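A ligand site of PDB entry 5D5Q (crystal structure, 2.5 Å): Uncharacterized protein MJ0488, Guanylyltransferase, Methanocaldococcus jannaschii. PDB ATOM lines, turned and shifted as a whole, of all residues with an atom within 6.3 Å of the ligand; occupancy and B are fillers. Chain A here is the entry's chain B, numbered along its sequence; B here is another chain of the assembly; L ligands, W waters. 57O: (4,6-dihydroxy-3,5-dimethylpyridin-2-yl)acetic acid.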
ATOM      1  N   ASP A  77     -24.241 -28.770  19.780  1.00  0.00           N
ATOM      2  CA  ASP A  77     -23.519 -29.216  20.976  1.00  0.00           C
ATOM      3  C   ASP A  77     -22.258 -30.032  20.673  1.00  0.00           C
ATOM      4  O   ASP A  77     -21.571 -30.475  21.594  1.00  0.00           O
ATOM      5  CB  ASP A  77     -24.449 -30.019  21.873  1.00  0.00           C
ATOM      6  CG  ASP A  77     -25.643 -29.219  22.349  1.00  0.00           C
ATOM      7  OD1 ASP A  77     -25.551 -27.974  22.389  1.00  0.00           O
ATOM      8  OD2 ASP A  77     -26.676 -29.834  22.693  1.00  0.00           O
ATOM      9  N   LYS A  86     -25.503 -21.989  17.596  1.00  0.00           N
ATOM     10  CA  LYS A  86     -26.954 -21.916  17.687  1.00  0.00           C
ATOM     11  C   LYS A  86     -27.429 -20.589  17.110  1.00  0.00           C
ATOM     12  O   LYS A  86     -28.343 -20.542  16.270  1.00  0.00           O
ATOM     13  CB  LYS A  86     -27.434 -22.051  19.133  1.00  0.00           C
ATOM     14  CG  LYS A  86     -27.248 -23.439  19.745  1.00  0.00           C
ATOM     15  CD  LYS A  86     -27.851 -23.504  21.144  1.00  0.00           C
ATOM     16  CE  LYS A  86     -27.558 -24.849  21.809  1.00  0.00           C
ATOM     17  NZ  LYS A  86     -28.413 -25.084  22.996  1.00  0.00           N
ATOM     18  N   ARG A 102     -28.404 -19.254  23.486  1.00  0.00           N
ATOM     19  CA  ARG A 102     -27.855 -19.649  24.764  1.00  0.00           C
ATOM     20  C   ARG A 102     -27.371 -21.093  24.684  1.00  0.00           C
ATOM     21  O   ARG A 102     -28.112 -21.955  24.222  1.00  0.00           O
ATOM     22  CB  ARG A 102     -28.901 -19.480  25.865  1.00  0.00           C
ATOM     23  CG  ARG A 102     -28.304 -19.349  27.240  1.00  0.00           C
ATOM     24  CD  ARG A 102     -28.146 -20.685  27.892  1.00  0.00           C
ATOM     25  NE  ARG A 102     -27.752 -20.565  29.285  1.00  0.00           N
ATOM     26  CZ  ARG A 102     -27.410 -21.602  30.038  1.00  0.00           C
ATOM     27  NH1 ARG A 102     -27.072 -21.432  31.309  1.00  0.00           N
ATOM     28  NH2 ARG A 102     -27.386 -22.819  29.504  1.00  0.00           N
ATOM     29  N   GLY A 103     -26.143 -21.350  25.122  1.00  0.00           N
ATOM     30  CA  GLY A 103     -25.634 -22.708  25.058  1.00  0.00           C
ATOM     31  C   GLY A 103     -24.376 -22.912  25.872  1.00  0.00           C
ATOM     32  O   GLY A 103     -24.058 -22.104  26.739  1.00  0.00           O
ATOM     33  N   ARG A 104     -23.654 -23.992  25.610  1.00  0.00           N
ATOM     34  CA  ARG A 104     -22.389 -24.227  26.281  1.00  0.00           C
ATOM     35  C   ARG A 104     -21.365 -23.254  25.725  1.00  0.00           C
ATOM     36  O   ARG A 104     -21.353 -22.974  24.524  1.00  0.00           O
ATOM     37  CB  ARG A 104     -21.930 -25.675  26.109  1.00  0.00           C
ATOM     38  CG  ARG A 104     -20.656 -26.031  26.860  1.00  0.00           C
ATOM     39  CD  ARG A 104     -20.365 -27.525  26.788  1.00  0.00           C
ATOM     40  NE  ARG A 104     -19.931 -27.939  25.457  1.00  0.00           N
ATOM     41  CZ  ARG A 104     -20.440 -28.984  24.811  1.00  0.00           C
ATOM     42  NH1 ARG A 104     -21.396 -29.721  25.358  1.00  0.00           N
ATOM     43  NH2 ARG A 104     -19.988 -29.301  23.603  1.00  0.00           N
ATOM     44  N   LEU A 105     -20.493 -22.732  26.591  1.00  0.00           N
ATOM     45  CA  LEU A 105     -19.480 -21.773  26.170  1.00  0.00           C
ATOM     46  C   LEU A 105     -18.535 -22.382  25.142  1.00  0.00           C
ATOM     47  O   LEU A 105     -18.446 -21.899  24.009  1.00  0.00           O
ATOM     48  CB  LEU A 105     -18.679 -21.272  27.380  1.00  0.00           C
ATOM     49  CG  LEU A 105     -17.458 -20.414  27.035  1.00  0.00           C
ATOM     50  CD1 LEU A 105     -17.890 -19.126  26.340  1.00  0.00           C
ATOM     51  CD2 LEU A 105     -16.645 -20.117  28.278  1.00  0.00           C
ATOM     52  N   ALA A 107     -15.809 -26.144  25.329  1.00  0.00           N
ATOM     53  CA  ALA A 107     -15.693 -27.580  25.574  1.00  0.00           C
ATOM     54  C   ALA A 107     -16.670 -28.024  26.667  1.00  0.00           C
ATOM     55  O   ALA A 107     -17.093 -27.213  27.490  1.00  0.00           O
ATOM     56  CB  ALA A 107     -14.258 -27.932  25.968  1.00  0.00           C
ATOM     57  N   PRO A 108     -17.041 -29.314  26.662  1.00  0.00           N
ATOM     58  CA  PRO A 108     -17.829 -29.874  27.767  1.00  0.00           C
ATOM     59  C   PRO A 108     -17.175 -29.609  29.124  1.00  0.00           C
ATOM     60  O   PRO A 108     -16.012 -29.954  29.321  1.00  0.00           O
ATOM     61  CB  PRO A 108     -17.857 -31.367  27.445  1.00  0.00           C
ATOM     62  CG  PRO A 108     -17.798 -31.420  25.965  1.00  0.00           C
ATOM     63  CD  PRO A 108     -16.905 -30.272  25.551  1.00  0.00           C
ATOM     64  N   GLY A 109     -17.919 -28.994  30.035  1.00  0.00           N
ATOM     65  CA  GLY A 109     -17.400 -28.652  31.353  1.00  0.00           C
ATOM     66  C   GLY A 109     -17.055 -27.177  31.508  1.00  0.00           C
ATOM     67  O   GLY A 109     -16.645 -26.746  32.581  1.00  0.00           O
ATOM     68  N   SER A 110     -17.210 -26.410  30.429  1.00  0.00           N
ATOM     69  CA  SER A 110     -16.755 -25.028  30.404  1.00  0.00           C
ATOM     70  C   SER A 110     -17.796 -23.997  30.832  1.00  0.00           C
ATOM     71  O   SER A 110     -17.561 -22.792  30.755  1.00  0.00           O
ATOM     72  CB  SER A 110     -16.261 -24.671  28.995  1.00  0.00           C
ATOM     73  OG  SER A 110     -17.305 -24.781  28.050  1.00  0.00           O
ATOM     74  N   GLY A 111     -18.960 -24.456  31.282  1.00  0.00           N
ATOM     75  CA  GLY A 111     -20.010 -23.548  31.704  1.00  0.00           C
ATOM     76  C   GLY A 111     -20.825 -23.044  30.523  1.00  0.00           C
ATOM     77  O   GLY A 111     -20.708 -23.576  29.424  1.00  0.00           O
ATOM     78  N   SER A 112     -21.638 -22.023  30.753  1.00  0.00           N
ATOM     79  CA  SER A 112     -22.565 -21.587  29.711  1.00  0.00           C
ATOM     80  C   SER A 112     -22.326 -20.157  29.225  1.00  0.00           C
ATOM     81  O   SER A 112     -21.685 -19.363  29.903  1.00  0.00           O
ATOM     82  CB  SER A 112     -24.012 -21.723  30.197  1.00  0.00           C
ATOM     83  OG  SER A 112     -24.332 -20.712  31.136  1.00  0.00           O
ATOM     84  N   MET A 113     -22.826 -19.868  28.039  1.00  0.00           N
ATOM     85  CA  MET A 113     -22.780 -18.536  27.447  1.00  0.00           C
ATOM     86  C   MET A 113     -24.120 -18.160  26.800  1.00  0.00           C
ATOM     87  O   MET A 113     -24.730 -18.973  26.099  1.00  0.00           O
ATOM     88  CB  MET A 113     -21.657 -18.447  26.409  1.00  0.00           C
ATOM     89  CG  MET A 113     -21.744 -17.207  25.530  1.00  0.00           C
ATOM     90  SD  MET A 113     -20.480 -17.109  24.259  1.00  0.00           S
ATOM     91  CE  MET A 113     -19.308 -15.985  25.027  1.00  0.00           C
ATOM     92  N   SER A 129     -21.822 -18.077  32.480  1.00  0.00           N
ATOM     93  CA  SER A 129     -22.149 -18.712  33.734  1.00  0.00           C
ATOM     94  C   SER A 129     -21.196 -19.850  34.037  1.00  0.00           C
ATOM     95  O   SER A 129     -20.713 -20.521  33.117  1.00  0.00           O
ATOM     96  CB  SER A 129     -23.575 -19.250  33.685  1.00  0.00           C
ATOM     97  OG  SER A 129     -24.484 -18.180  33.554  1.00  0.00           O
ATOM     98  N   PRO A 130     -20.927 -20.093  35.337  1.00  0.00           N
ATOM     99  CA  PRO A 130     -20.112 -21.222  35.762  1.00  0.00           C
ATOM    100  C   PRO A 130     -20.721 -22.539  35.288  1.00  0.00           C
ATOM    101  O   PRO A 130     -21.889 -22.542  34.885  1.00  0.00           O
ATOM    102  CB  PRO A 130     -20.134 -21.125  37.292  1.00  0.00           C
ATOM    103  CG  PRO A 130     -20.413 -19.694  37.565  1.00  0.00           C
ATOM    104  CD  PRO A 130     -21.320 -19.235  36.466  1.00  0.00           C
ATOM    105  N   SER A 131     -19.950 -23.617  35.313  1.00  0.00           N
ATOM    106  CA  SER A 131     -20.478 -24.917  34.941  1.00  0.00           C
ATOM    107  C   SER A 131     -21.713 -25.247  35.783  1.00  0.00           C
ATOM    108  O   SER A 131     -21.736 -24.977  36.987  1.00  0.00           O
ATOM    109  CB  SER A 131     -19.409 -25.997  35.106  1.00  0.00           C
ATOM    110  OG  SER A 131     -19.885 -27.260  34.669  1.00  0.00           O
ATOM    111  N   SER A 132     -22.729 -25.824  35.157  1.00  0.00           N
ATOM    112  CA  SER A 132     -23.944 -26.213  35.854  1.00  0.00           C
ATOM    113  C   SER A 132     -23.619 -27.255  36.919  1.00  0.00           C
ATOM    114  O   SER A 132     -24.392 -27.470  37.854  1.00  0.00           O
ATOM    115  CB  SER A 132     -24.990 -26.768  34.883  1.00  0.00           C
ATOM    116  OG  SER A 132     -24.471 -27.884  34.177  1.00  0.00           O
ATOM    117  N   VAL A 133     -22.472 -27.899  36.758  1.00  0.00           N
ATOM    118  CA  VAL A 133     -21.956 -28.821  37.732  1.00  0.00           C
ATOM    119  C   VAL A 133     -21.706 -28.082  39.046  1.00  0.00           C
ATOM    120  O   VAL A 133     -21.951 -28.617  40.136  1.00  0.00           O
ATOM    121  CB  VAL A 133     -20.664 -29.491  37.242  1.00  0.00           C
ATOM    122  CG1 VAL A 133     -20.077 -30.315  38.344  1.00  0.00           C
ATOM    123  CG2 VAL A 133     -20.940 -30.357  36.031  1.00  0.00           C
ATOM    124  N   HIS A 135     -22.832 -24.573  39.829  1.00  0.00           N
ATOM    125  CA  HIS A 135     -23.883 -23.692  40.322  1.00  0.00           C
ATOM    126  C   HIS A 135     -25.241 -24.335  40.478  1.00  0.00           C
ATOM    127  O   HIS A 135     -26.194 -23.628  40.787  1.00  0.00           O
ATOM    128  CB  HIS A 135     -24.022 -22.460  39.396  1.00  0.00           C
ATOM    129  CG  HIS A 135     -24.649 -22.750  38.079  1.00  0.00           C
ATOM    130  ND1 HIS A 135     -26.012 -23.014  37.925  1.00  0.00           N
ATOM    131  CD2 HIS A 135     -24.148 -22.792  36.823  1.00  0.00           C
ATOM    132  CE1 HIS A 135     -26.292 -23.226  36.670  1.00  0.00           C
ATOM    133  NE2 HIS A 135     -25.162 -23.090  35.960  1.00  0.00           N
ATOM    134  N   ILE A 139     -31.531 -24.180  34.315  1.00  0.00           N
ATOM    135  CA  ILE A 139     -31.496 -23.305  33.152  1.00  0.00           C
ATOM    136  C   ILE A 139     -32.275 -21.936  33.132  1.00  0.00           C
ATOM    137  O   ILE A 139     -31.808 -20.998  32.479  1.00  0.00           O
ATOM    138  CB  ILE A 139     -31.914 -24.178  31.969  1.00  0.00           C
ATOM    139  CG1 ILE A 139     -30.739 -25.089  31.568  1.00  0.00           C
ATOM    140  CG2 ILE A 139     -32.366 -23.389  30.787  1.00  0.00           C
ATOM    141  CD1 ILE A 139     -29.562 -24.319  31.286  1.00  0.00           C
ATOM    142  N   ALA B  11     -19.300 -37.208  25.957  1.00  0.00           N
ATOM    143  CA  ALA B  11     -20.249 -36.108  25.928  1.00  0.00           C
ATOM    144  C   ALA B  11     -20.963 -36.018  24.575  1.00  0.00           C
ATOM    145  O   ALA B  11     -22.196 -35.875  24.509  1.00  0.00           O
ATOM    146  CB  ALA B  11     -19.561 -34.791  26.249  1.00  0.00           C
ATOM    147  N   SER B  15     -24.830 -36.387  23.366  1.00  0.00           N
ATOM    148  CA  SER B  15     -25.558 -35.383  22.591  1.00  0.00           C
ATOM    149  C   SER B  15     -26.222 -36.010  21.362  1.00  0.00           C
ATOM    150  O   SER B  15     -27.356 -35.675  21.021  1.00  0.00           O
ATOM    151  CB  SER B  15     -24.628 -34.251  22.161  1.00  0.00           C
ATOM    152  OG  SER B  15     -24.321 -33.397  23.242  1.00  0.00           O
ATOM    153  N   ARG B  20     -28.038 -35.959  26.576  1.00  0.00           N
ATOM    154  CA  ARG B  20     -27.150 -35.026  27.246  1.00  0.00           C
ATOM    155  C   ARG B  20     -27.852 -33.942  28.074  1.00  0.00           C
ATOM    156  O   ARG B  20     -28.721 -33.233  27.564  1.00  0.00           O
ATOM    157  CB  ARG B  20     -26.260 -34.339  26.197  1.00  0.00           C
ATOM    158  CG  ARG B  20     -25.347 -33.244  26.709  1.00  0.00           C
ATOM    159  CD  ARG B  20     -24.041 -33.781  27.272  1.00  0.00           C
ATOM    160  NE  ARG B  20     -23.149 -32.686  27.658  1.00  0.00           N
ATOM    161  CZ  ARG B  20     -22.040 -32.838  28.369  1.00  0.00           C
ATOM    162  NH1 ARG B  20     -21.669 -34.047  28.787  1.00  0.00           N
ATOM    163  NH2 ARG B  20     -21.287 -31.785  28.661  1.00  0.00           N
ATOM    164  N   ARG B  21     -27.484 -33.825  29.349  1.00  0.00           N
ATOM    165  CA  ARG B  21     -27.975 -32.728  30.180  1.00  0.00           C
ATOM    166  C   ARG B  21     -26.808 -31.919  30.730  1.00  0.00           C
ATOM    167  O   ARG B  21     -26.271 -32.250  31.792  1.00  0.00           O
ATOM    168  CB  ARG B  21     -28.849 -33.209  31.343  1.00  0.00           C
ATOM    169  CG  ARG B  21     -29.255 -32.036  32.251  1.00  0.00           C
ATOM    170  CD  ARG B  21     -30.144 -32.405  33.434  1.00  0.00           C
ATOM    171  NE  ARG B  21     -30.299 -33.844  33.617  1.00  0.00           N
ATOM    172  CZ  ARG B  21     -31.385 -34.522  33.245  1.00  0.00           C
ATOM    173  NH1 ARG B  21     -32.404 -33.883  32.677  1.00  0.00           N
ATOM    174  NH2 ARG B  21     -31.456 -35.829  33.457  1.00  0.00           N
ATOM    175  N   GLY B  22     -26.415 -30.887  30.000  1.00  0.00           N
ATOM    176  CA  GLY B  22     -25.337 -30.022  30.443  1.00  0.00           C
ATOM    177  C   GLY B  22     -24.025 -30.684  30.781  1.00  0.00           C
ATOM    178  O   GLY B  22     -23.794 -31.861  30.478  1.00  0.00           O
ATOM    179  N   ASP B  23     -23.157 -29.921  31.431  1.00  0.00           N
ATOM    180  CA  ASP B  23     -21.834 -30.352  31.821  1.00  0.00           C
ATOM    181  C   ASP B  23     -21.812 -31.499  32.835  1.00  0.00           C
ATOM    182  O   ASP B  23     -22.710 -31.630  33.660  1.00  0.00           O
ATOM    183  CB  ASP B  23     -21.053 -29.176  32.393  1.00  0.00           C
ATOM    184  CG  ASP B  23     -20.622 -28.193  31.318  1.00  0.00           C
ATOM    185  OD1 ASP B  23     -20.585 -28.600  30.137  1.00  0.00           O
ATOM    186  OD2 ASP B  23     -20.321 -27.031  31.662  1.00  0.00           O
ATOM    187  N   LYS B  24     -20.760 -32.309  32.757  1.00  0.00           N
ATOM    188  CA  LYS B  24     -20.553 -33.392  33.692  1.00  0.00           C
ATOM    189  C   LYS B  24     -19.350 -33.069  34.574  1.00  0.00           C
ATOM    190  O   LYS B  24     -18.434 -32.348  34.177  1.00  0.00           O
ATOM    191  CB  LYS B  24     -20.311 -34.723  32.978  1.00  0.00           C
ATOM    192  CG  LYS B  24     -21.512 -35.307  32.263  1.00  0.00           C
ATOM    193  CD  LYS B  24     -21.319 -36.801  32.055  1.00  0.00           C
ATOM    194  CE  LYS B  24     -22.614 -37.534  31.842  1.00  0.00           C
ATOM    195  NZ  LYS B  24     -23.630 -37.262  32.888  1.00  0.00           N
ATOM    196  N   GLU B  27     -15.929 -33.783  33.296  1.00  0.00           N
ATOM    197  CA  GLU B  27     -15.528 -32.816  32.286  1.00  0.00           C
ATOM    198  C   GLU B  27     -14.868 -31.620  32.944  1.00  0.00           C
ATOM    199  O   GLU B  27     -13.759 -31.202  32.595  1.00  0.00           O
ATOM    200  CB  GLU B  27     -16.733 -32.393  31.457  1.00  0.00           C
ATOM    201  CG  GLU B  27     -17.350 -33.540  30.664  1.00  0.00           C
ATOM    202  CD  GLU B  27     -18.764 -33.262  30.202  1.00  0.00           C
ATOM    203  OE1 GLU B  27     -19.232 -32.121  30.347  1.00  0.00           O
ATOM    204  OE2 GLU B  27     -19.413 -34.202  29.689  1.00  0.00           O
HETATM  205  CAA 57O L   1     -25.286 -29.285  26.331  1.00  0.00           C
HETATM  206  CAB 57O L   1     -25.448 -25.099  28.698  1.00  0.00           C
HETATM  207  OAE 57O L   1     -22.986 -29.884  27.659  1.00  0.00           O
HETATM  208  CAM 57O L   1     -23.648 -26.646  29.100  1.00  0.00           C
HETATM  209  OAD 57O L   1     -23.872 -27.373  31.591  1.00  0.00           O
HETATM  210  OAC 57O L   1     -22.910 -25.523  32.380  1.00  0.00           O
HETATM  211  CAI 57O L   1     -23.306 -26.262  31.450  1.00  0.00           C
HETATM  212  CAG 57O L   1     -23.076 -25.777  30.025  1.00  0.00           C
HETATM  213  NAH 57O L   1     -23.054 -27.823  28.826  1.00  0.00           N
HETATM  214  CAL 57O L   1     -23.574 -28.683  27.933  1.00  0.00           C
HETATM  215  CAJ 57O L   1     -24.746 -28.397  27.252  1.00  0.00           C
HETATM  216  CAN 57O L   1     -25.362 -27.185  27.522  1.00  0.00           C
HETATM  217  OAF 57O L   1     -26.512 -26.859  26.877  1.00  0.00           O
HETATM  218  CAK 57O L   1     -24.822 -26.297  28.443  1.00  0.00           C
HETATM  219  O   HOH W   1     -28.719 -24.597  26.875  1.00  0.00           O
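Residues that only touch the ligand: Arg 102 (3.1 Å), Gly 22 of chain B (3.2 Å), Gly 111 (3.3 Å), Ser 131 (3.6 Å), Gly 103 (3.7 Å), Asp 77 (3.9 Å) and Ser 112 (3.96 Å). The nearest printed residue that does not touch the ligand is Pro 130 (4.03 Å).
The side-chain carboxylate (OD2) of Asp 23 of chain B sits close to an oxygen (OAC) of the ligand, 3.1 Å away. The backbone NH (N) of Ser 132 sits at hydrogen-bond distance from an oxygen (OAC) of the ligand, 2.8 Å away. The backbone NH of Asp 23 of chain B is in hydrogen-bond range of an oxygen (OAD) of the ligand, at 2.7 Å. OG of Ser 132 lies within hydrogen-bond range of OAD of the ligand (2.7 Å). NH1 of Arg 104 sits at hydrogen-bond distance from OAE of the ligand (2.8 Å). The guanidinium group (NH2) of Arg 20 of chain B sits at hydrogen-bond distance from an oxygen (OAE) of the ligand.
Water W1 bridges an oxygen (OAF) of the ligand and the guanidinium group of Arg 102.
The backbone carbonyl oxygen (O) of Arg 102 sits at hydrogen-bond distance from the side-chain amino group (NZ) of Lys 86, at 3.4 Å. The side-chain carboxylate (OD1) of Asp 23 of chain B lies within hydrogen-bond range of the backbone NH (N) of Gly 109, 2.7 Å away. The backbone carbonyl oxygen (O) of Gly 103 is in hydrogen-bond range of the backbone NH (N) of Met 113, at 2.9 Å. The side-chain carboxylate of Asp 23 of chain B lies within hydrogen-bond range of the side-chain hydroxyl of Ser 131 (3.0 Å). The side-chain carboxylate (OE2) of Glu 27 of chain B lies within salt-bridge range of the guanidinium group (NH1) of Arg 20 of chain B (2.4 Å). The side-chain hydroxyl (OG) of Ser 131 lies close to the backbone NH (N) of Val 133 (3.4 Å). N of Leu 105 is in hydrogen-bond range of O of Gly 111. O of Gly 22 of chain B lies close to NE of Arg 20 of chain B.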
